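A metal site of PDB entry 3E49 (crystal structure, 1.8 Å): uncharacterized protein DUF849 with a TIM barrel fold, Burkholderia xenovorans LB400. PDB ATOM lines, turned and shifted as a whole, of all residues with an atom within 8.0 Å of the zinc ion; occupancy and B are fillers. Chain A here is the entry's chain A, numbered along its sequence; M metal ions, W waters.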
ATOM      1  N   ALA A  13      17.333 -24.425 -12.168  1.00  0.00           N
ATOM      2  CA  ALA A  13      18.481 -23.534 -12.013  1.00  0.00           C
ATOM      3  C   ALA A  13      19.424 -23.924 -13.153  1.00  0.00           C
ATOM      4  O   ALA A  13      20.150 -24.931 -13.067  1.00  0.00           O
ATOM      5  CB  ALA A  13      19.144 -23.777 -10.663  1.00  0.00           C
ATOM      6  N   VAL A  14      19.461 -23.090 -14.188  1.00  0.00           N
ATOM      7  CA  VAL A  14      20.101 -23.487 -15.453  1.00  0.00           C
ATOM      8  C   VAL A  14      21.629 -23.514 -15.555  1.00  0.00           C
ATOM      9  O   VAL A  14      22.128 -24.242 -16.391  1.00  0.00           O
ATOM     10  CB  VAL A  14      19.536 -22.674 -16.673  1.00  0.00           C
ATOM     11  CG1 VAL A  14      18.051 -22.957 -16.859  1.00  0.00           C
ATOM     12  CG2 VAL A  14      19.797 -21.200 -16.491  1.00  0.00           C
ATOM     13  N   THR A  15      22.342 -22.719 -14.767  1.00  0.00           N
ATOM     14  CA  THR A  15      23.835 -22.720 -14.843  1.00  0.00           C
ATOM     15  C   THR A  15      24.586 -22.398 -13.552  1.00  0.00           C
ATOM     16  O   THR A  15      25.626 -23.029 -13.217  1.00  0.00           O
ATOM     17  CB  THR A  15      24.312 -21.808 -16.000  1.00  0.00           C
ATOM     18  OG1 THR A  15      25.694 -22.073 -16.274  1.00  0.00           O
ATOM     19  CG2 THR A  15      24.081 -20.314 -15.662  1.00  0.00           C
ATOM     20  N   GLY A  16      24.087 -21.415 -12.803  1.00  0.00           N
ATOM     21  CA  GLY A  16      24.682 -21.035 -11.534  1.00  0.00           C
ATOM     22  C   GLY A  16      26.113 -20.476 -11.607  1.00  0.00           C
ATOM     23  O   GLY A  16      26.505 -19.992 -12.644  1.00  0.00           O
ATOM     24  N   ALA A  17      26.865 -20.616 -10.517  1.00  0.00           N
ATOM     25  CA  ALA A  17      28.257 -20.120 -10.421  1.00  0.00           C
ATOM     26  C   ALA A  17      29.170 -21.155  -9.797  1.00  0.00           C
ATOM     27  O   ALA A  17      30.327 -20.856  -9.584  1.00  0.00           O
ATOM     28  CB  ALA A  17      28.294 -18.927  -9.542  1.00  0.00           C
ATOM     29  N   ILE A  18      28.647 -22.332  -9.444  1.00  0.00           N
ATOM     30  CA  ILE A  18      29.499 -23.325  -8.765  1.00  0.00           C
ATOM     31  C   ILE A  18      30.318 -24.161  -9.746  1.00  0.00           C
ATOM     32  O   ILE A  18      31.576 -24.214  -9.674  1.00  0.00           O
ATOM     33  CB  ILE A  18      28.673 -24.208  -7.804  1.00  0.00           C
ATOM     34  CG1 ILE A  18      28.465 -23.424  -6.504  1.00  0.00           C
ATOM     35  CG2 ILE A  18      29.434 -25.464  -7.473  1.00  0.00           C
ATOM     36  CD1 ILE A  18      27.546 -24.111  -5.465  1.00  0.00           C
ATOM     37  N   HIS A  50      15.693 -20.266 -12.379  1.00  0.00           N
ATOM     38  CA  HIS A  50      16.645 -19.628 -11.497  1.00  0.00           C
ATOM     39  C   HIS A  50      17.900 -19.349 -12.337  1.00  0.00           C
ATOM     40  O   HIS A  50      18.536 -20.281 -12.880  1.00  0.00           O
ATOM     41  CB  HIS A  50      16.904 -20.535 -10.283  1.00  0.00           C
ATOM     42  CG  HIS A  50      17.998 -20.066  -9.387  1.00  0.00           C
ATOM     43  ND1 HIS A  50      17.781 -19.563  -8.127  1.00  0.00           N
ATOM     44  CD2 HIS A  50      19.342 -20.165  -9.511  1.00  0.00           C
ATOM     45  CE1 HIS A  50      18.926 -19.298  -7.548  1.00  0.00           C
ATOM     46  NE2 HIS A  50      19.896 -19.569  -8.396  1.00  0.00           N
ATOM     47  N   LEU A  51      18.261 -18.067 -12.400  1.00  0.00           N
ATOM     48  CA  LEU A  51      19.289 -17.566 -13.327  1.00  0.00           C
ATOM     49  C   LEU A  51      20.494 -16.883 -12.769  1.00  0.00           C
ATOM     50  O   LEU A  51      20.418 -16.075 -11.833  1.00  0.00           O
ATOM     51  CB  LEU A  51      18.611 -16.576 -14.317  1.00  0.00           C
ATOM     52  CG  LEU A  51      17.619 -17.205 -15.287  1.00  0.00           C
ATOM     53  CD1 LEU A  51      16.536 -16.226 -15.752  1.00  0.00           C
ATOM     54  CD2 LEU A  51      18.331 -17.834 -16.477  1.00  0.00           C
ATOM     55  N   HIS A  52      21.650 -17.273 -13.342  1.00  0.00           N
ATOM     56  CA  HIS A  52      22.901 -16.551 -13.159  1.00  0.00           C
ATOM     57  C   HIS A  52      23.397 -16.267 -14.577  1.00  0.00           C
ATOM     58  O   HIS A  52      22.923 -16.864 -15.554  1.00  0.00           O
ATOM     59  CB  HIS A  52      24.014 -17.373 -12.501  1.00  0.00           C
ATOM     60  CG  HIS A  52      23.761 -17.759 -11.090  1.00  0.00           C
ATOM     61  ND1 HIS A  52      24.718 -17.630 -10.104  1.00  0.00           N
ATOM     62  CD2 HIS A  52      22.701 -18.387 -10.506  1.00  0.00           C
ATOM     63  CE1 HIS A  52      24.260 -18.136  -8.973  1.00  0.00           C
ATOM     64  NE2 HIS A  52      23.045 -18.605  -9.187  1.00  0.00           N
ATOM     65  N   ASN A  84      13.798 -15.835 -12.095  1.00  0.00           N
ATOM     66  CA  ASN A  84      14.275 -15.703 -10.752  1.00  0.00           C
ATOM     67  C   ASN A  84      15.780 -15.406 -10.825  1.00  0.00           C
ATOM     68  O   ASN A  84      16.527 -16.227 -11.299  1.00  0.00           O
ATOM     69  CB  ASN A  84      13.986 -17.035 -10.052  1.00  0.00           C
ATOM     70  CG  ASN A  84      14.535 -17.117  -8.659  1.00  0.00           C
ATOM     71  OD1 ASN A  84      15.286 -16.262  -8.185  1.00  0.00           O
ATOM     72  ND2 ASN A  84      14.180 -18.213  -7.976  1.00  0.00           N
ATOM     73  N   LEU A  85      16.202 -14.231 -10.398  1.00  0.00           N
ATOM     74  CA  LEU A  85      17.631 -13.854 -10.437  1.00  0.00           C
ATOM     75  C   LEU A  85      18.358 -14.046  -9.142  1.00  0.00           C
ATOM     76  O   LEU A  85      17.846 -13.714  -8.098  1.00  0.00           O
ATOM     77  CB  LEU A  85      17.796 -12.376 -10.767  1.00  0.00           C
ATOM     78  CG  LEU A  85      17.108 -11.956 -12.060  1.00  0.00           C
ATOM     79  CD1 LEU A  85      17.445 -10.475 -12.352  1.00  0.00           C
ATOM     80  CD2 LEU A  85      17.484 -12.907 -13.212  1.00  0.00           C
ATOM     81  N   THR A  86      19.596 -14.518  -9.252  1.00  0.00           N
ATOM     82  CA  THR A  86      20.444 -14.705  -8.102  1.00  0.00           C
ATOM     83  C   THR A  86      20.923 -13.374  -7.491  1.00  0.00           C
ATOM     84  O   THR A  86      21.078 -12.393  -8.215  1.00  0.00           O
ATOM     85  CB  THR A  86      21.701 -15.525  -8.478  1.00  0.00           C
ATOM     86  OG1 THR A  86      22.467 -15.723  -7.305  1.00  0.00           O
ATOM     87  CG2 THR A  86      22.582 -14.805  -9.521  1.00  0.00           C
ATOM     88  N   THR A  87      21.084 -13.355  -6.160  1.00  0.00           N
ATOM     89  CA  THR A  87      21.681 -12.238  -5.432  1.00  0.00           C
ATOM     90  C   THR A  87      22.975 -12.699  -4.809  1.00  0.00           C
ATOM     91  O   THR A  87      23.567 -11.993  -4.015  1.00  0.00           O
ATOM     92  CB  THR A  87      20.786 -11.659  -4.325  1.00  0.00           C
ATOM     93  OG1 THR A  87      20.580 -12.575  -3.228  1.00  0.00           O
ATOM     94  CG2 THR A  87      19.509 -11.225  -4.898  1.00  0.00           C
ATOM     95  N   GLY A  88      23.392 -13.908  -5.140  1.00  0.00           N
ATOM     96  CA  GLY A  88      24.625 -14.464  -4.594  1.00  0.00           C
ATOM     97  C   GLY A  88      25.648 -14.372  -5.680  1.00  0.00           C
ATOM     98  O   GLY A  88      26.615 -13.566  -5.603  1.00  0.00           O
ATOM     99  N   GLY A  89      25.363 -15.125  -6.747  1.00  0.00           N
ATOM    100  CA  GLY A  89      26.225 -15.244  -7.903  1.00  0.00           C
ATOM    101  C   GLY A  89      27.395 -16.076  -7.401  1.00  0.00           C
ATOM    102  O   GLY A  89      27.204 -17.177  -6.848  1.00  0.00           O
ATOM    103  N   SER A  90      28.602 -15.547  -7.568  1.00  0.00           N
ATOM    104  CA  SER A  90      29.780 -16.192  -7.062  1.00  0.00           C
ATOM    105  C   SER A  90      30.022 -15.762  -5.609  1.00  0.00           C
ATOM    106  O   SER A  90      29.973 -14.555  -5.298  1.00  0.00           O
ATOM    107  CB  SER A  90      30.996 -15.842  -7.934  1.00  0.00           C
ATOM    108  OG  SER A  90      32.201 -16.346  -7.386  1.00  0.00           O
ATOM    109  N   SER A 111      16.874 -14.922  -5.601  1.00  0.00           N
ATOM    110  CA  SER A 111      17.317 -15.886  -4.599  1.00  0.00           C
ATOM    111  C   SER A 111      17.897 -15.081  -3.452  1.00  0.00           C
ATOM    112  O   SER A 111      18.386 -13.970  -3.663  1.00  0.00           O
ATOM    113  CB  SER A 111      18.351 -16.840  -5.184  1.00  0.00           C
ATOM    114  OG  SER A 111      19.570 -16.169  -5.456  1.00  0.00           O
ATOM    115  N   GLU A 170      13.257 -16.442  -3.144  1.00  0.00           N
ATOM    116  CA  GLU A 170      13.501 -17.860  -3.019  1.00  0.00           C
ATOM    117  C   GLU A 170      14.549 -17.861  -1.897  1.00  0.00           C
ATOM    118  O   GLU A 170      15.715 -17.519  -2.138  1.00  0.00           O
ATOM    119  CB  GLU A 170      14.075 -18.480  -4.321  1.00  0.00           C
ATOM    120  CG  GLU A 170      14.467 -19.958  -4.219  1.00  0.00           C
ATOM    121  CD  GLU A 170      15.325 -20.451  -5.374  1.00  0.00           C
ATOM    122  OE1 GLU A 170      15.900 -19.638  -6.107  1.00  0.00           O
ATOM    123  OE2 GLU A 170      15.481 -21.697  -5.529  1.00  0.00           O
ATOM    124  N   GLU A 172      17.086 -19.421   0.224  1.00  0.00           N
ATOM    125  CA  GLU A 172      17.950 -20.572   0.101  1.00  0.00           C
ATOM    126  C   GLU A 172      18.477 -20.855   1.476  1.00  0.00           C
ATOM    127  O   GLU A 172      19.276 -20.085   2.007  1.00  0.00           O
ATOM    128  CB  GLU A 172      19.085 -20.291  -0.862  1.00  0.00           C
ATOM    129  CG  GLU A 172      18.610 -20.157  -2.264  1.00  0.00           C
ATOM    130  CD  GLU A 172      19.733 -19.777  -3.230  1.00  0.00           C
ATOM    131  OE1 GLU A 172      20.634 -18.980  -2.815  1.00  0.00           O
ATOM    132  OE2 GLU A 172      19.674 -20.275  -4.380  1.00  0.00           O
ATOM    133  N   TYR A 174      20.449 -23.432   3.694  1.00  0.00           N
ATOM    134  CA  TYR A 174      21.386 -24.557   3.668  1.00  0.00           C
ATOM    135  C   TYR A 174      21.557 -25.338   4.957  1.00  0.00           C
ATOM    136  O   TYR A 174      22.338 -26.314   5.005  1.00  0.00           O
ATOM    137  CB  TYR A 174      22.780 -24.035   3.267  1.00  0.00           C
ATOM    138  CG  TYR A 174      22.838 -23.414   1.896  1.00  0.00           C
ATOM    139  CD1 TYR A 174      22.324 -22.144   1.665  1.00  0.00           C
ATOM    140  CD2 TYR A 174      23.436 -24.088   0.852  1.00  0.00           C
ATOM    141  CE1 TYR A 174      22.403 -21.560   0.397  1.00  0.00           C
ATOM    142  CE2 TYR A 174      23.527 -23.519  -0.404  1.00  0.00           C
ATOM    143  CZ  TYR A 174      23.003 -22.254  -0.622  1.00  0.00           C
ATOM    144  OH  TYR A 174      23.115 -21.731  -1.874  1.00  0.00           O
ATOM    145  N   LEU A 234      16.200 -28.820  -2.906  1.00  0.00           N
ATOM    146  CA  LEU A 234      17.325 -28.778  -3.793  1.00  0.00           C
ATOM    147  C   LEU A 234      18.364 -29.757  -3.241  1.00  0.00           C
ATOM    148  O   LEU A 234      18.917 -29.516  -2.199  1.00  0.00           O
ATOM    149  CB  LEU A 234      17.963 -27.402  -3.806  1.00  0.00           C
ATOM    150  CG  LEU A 234      19.004 -27.053  -4.890  1.00  0.00           C
ATOM    151  CD1 LEU A 234      19.556 -25.640  -4.604  1.00  0.00           C
ATOM    152  CD2 LEU A 234      20.155 -28.057  -4.961  1.00  0.00           C
ATOM    153  N   ARG A 255      13.390 -28.649  -7.115  1.00  0.00           N
ATOM    154  CA  ARG A 255      14.360 -27.856  -7.877  1.00  0.00           C
ATOM    155  C   ARG A 255      15.331 -28.787  -8.535  1.00  0.00           C
ATOM    156  O   ARG A 255      15.876 -29.673  -7.882  1.00  0.00           O
ATOM    157  CB  ARG A 255      15.103 -26.841  -7.028  1.00  0.00           C
ATOM    158  CG  ARG A 255      16.198 -26.116  -7.751  1.00  0.00           C
ATOM    159  CD  ARG A 255      16.661 -24.923  -7.007  1.00  0.00           C
ATOM    160  NE  ARG A 255      17.977 -24.528  -7.461  1.00  0.00           N
ATOM    161  CZ  ARG A 255      18.631 -23.456  -7.050  1.00  0.00           C
ATOM    162  NH1 ARG A 255      18.070 -22.562  -6.257  1.00  0.00           N
ATOM    163  NH2 ARG A 255      19.855 -23.256  -7.471  1.00  0.00           N
ATOM    164  N   GLU A 259      22.948 -26.116 -12.710  1.00  0.00           N
ATOM    165  CA  GLU A 259      23.575 -25.330 -11.661  1.00  0.00           C
ATOM    166  C   GLU A 259      23.914 -26.225 -10.455  1.00  0.00           C
ATOM    167  O   GLU A 259      24.935 -26.050  -9.835  1.00  0.00           O
ATOM    168  CB  GLU A 259      22.639 -24.233 -11.151  1.00  0.00           C
ATOM    169  CG  GLU A 259      23.105 -23.622  -9.844  1.00  0.00           C
ATOM    170  CD  GLU A 259      22.502 -22.289  -9.476  1.00  0.00           C
ATOM    171  OE1 GLU A 259      21.851 -21.626 -10.319  1.00  0.00           O
ATOM    172  OE2 GLU A 259      22.729 -21.914  -8.308  1.00  0.00           O
ATOM    173  N   ASP A 260      22.977 -27.137 -10.149  1.00  0.00           N
ATOM    174  CA  ASP A 260      22.967 -27.988  -8.954  1.00  0.00           C
ATOM    175  C   ASP A 260      23.560 -29.373  -9.156  1.00  0.00           C
ATOM    176  O   ASP A 260      24.174 -29.909  -8.244  1.00  0.00           O
ATOM    177  CB  ASP A 260      21.511 -28.169  -8.490  1.00  0.00           C
ATOM    178  CG  ASP A 260      20.775 -26.832  -8.241  1.00  0.00           C
ATOM    179  OD1 ASP A 260      21.427 -25.817  -7.931  1.00  0.00           O
ATOM    180  OD2 ASP A 260      19.537 -26.785  -8.359  1.00  0.00           O
HETATM  181 ZN    ZN M   1      21.956 -19.945  -7.765  1.00  0.00          ZN
HETATM  182  O   HOH W   1      24.099 -19.774  -6.132  1.00  0.00           O
HETATM  183  O   HOH W   2      21.373 -21.043  -5.722  1.00  0.00           O
HETATM  184  O   HOH W   3      21.867 -18.259  -6.102  1.00  0.00           O
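The guanidinium group (NH2) of Arg 255 lies within salt-bridge range of the side-chain carboxylate (OE1) of Glu 259, 3.8 Å away.
The backbone NH (N) of Gly 16 sits close to the side-chain carboxylate (OE1) of Glu 259 (3.3 Å).
N of Glu 259 sits at hydrogen-bond distance from O of Ala 13, 3.1 Å away.
ND1 of His 50 is in hydrogen-bond range of OE1 of Glu 170, 2.8 Å away.
The backbone NH (N) of Val 14 is in hydrogen-bond range of the backbone carbonyl oxygen (O) of His 50 (3.2 Å).
A ring nitrogen (NE2) of His 52 lies close to the side-chain hydroxyl (OG1) of Thr 86, at 3.5 Å.
OE2 of Glu 172 is in salt-bridge range of NH1 of Arg 255, at 3.4 Å.
The side-chain carboxylate (OD2) of Asp 260 lies within salt-bridge range of the guanidinium group (NE) of Arg 255, at 2.9 Å.
NH2 of Arg 255 touches the zinc ion (3.9 Å).
Within 4 Å of the zinc ion: His 50, His 52, Arg 255 and Glu 259.
The zinc ion is bound by OE2 of Glu 259 (2.2 Å), NE2 of His 50 (2.2 Å), NE2 of His 52 (2.2 Å), water W3 (2.4 Å) and water W2 (2.4 Å).
The zinc ion has five donor atoms within binding distance.
Slightly farther from the zinc ion lies water W1 (2.7 Å).
Water W3 lies within hydrogen-bond range of OG1 of Thr 86, OG of Ser 111 and OE2 of Glu 172.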
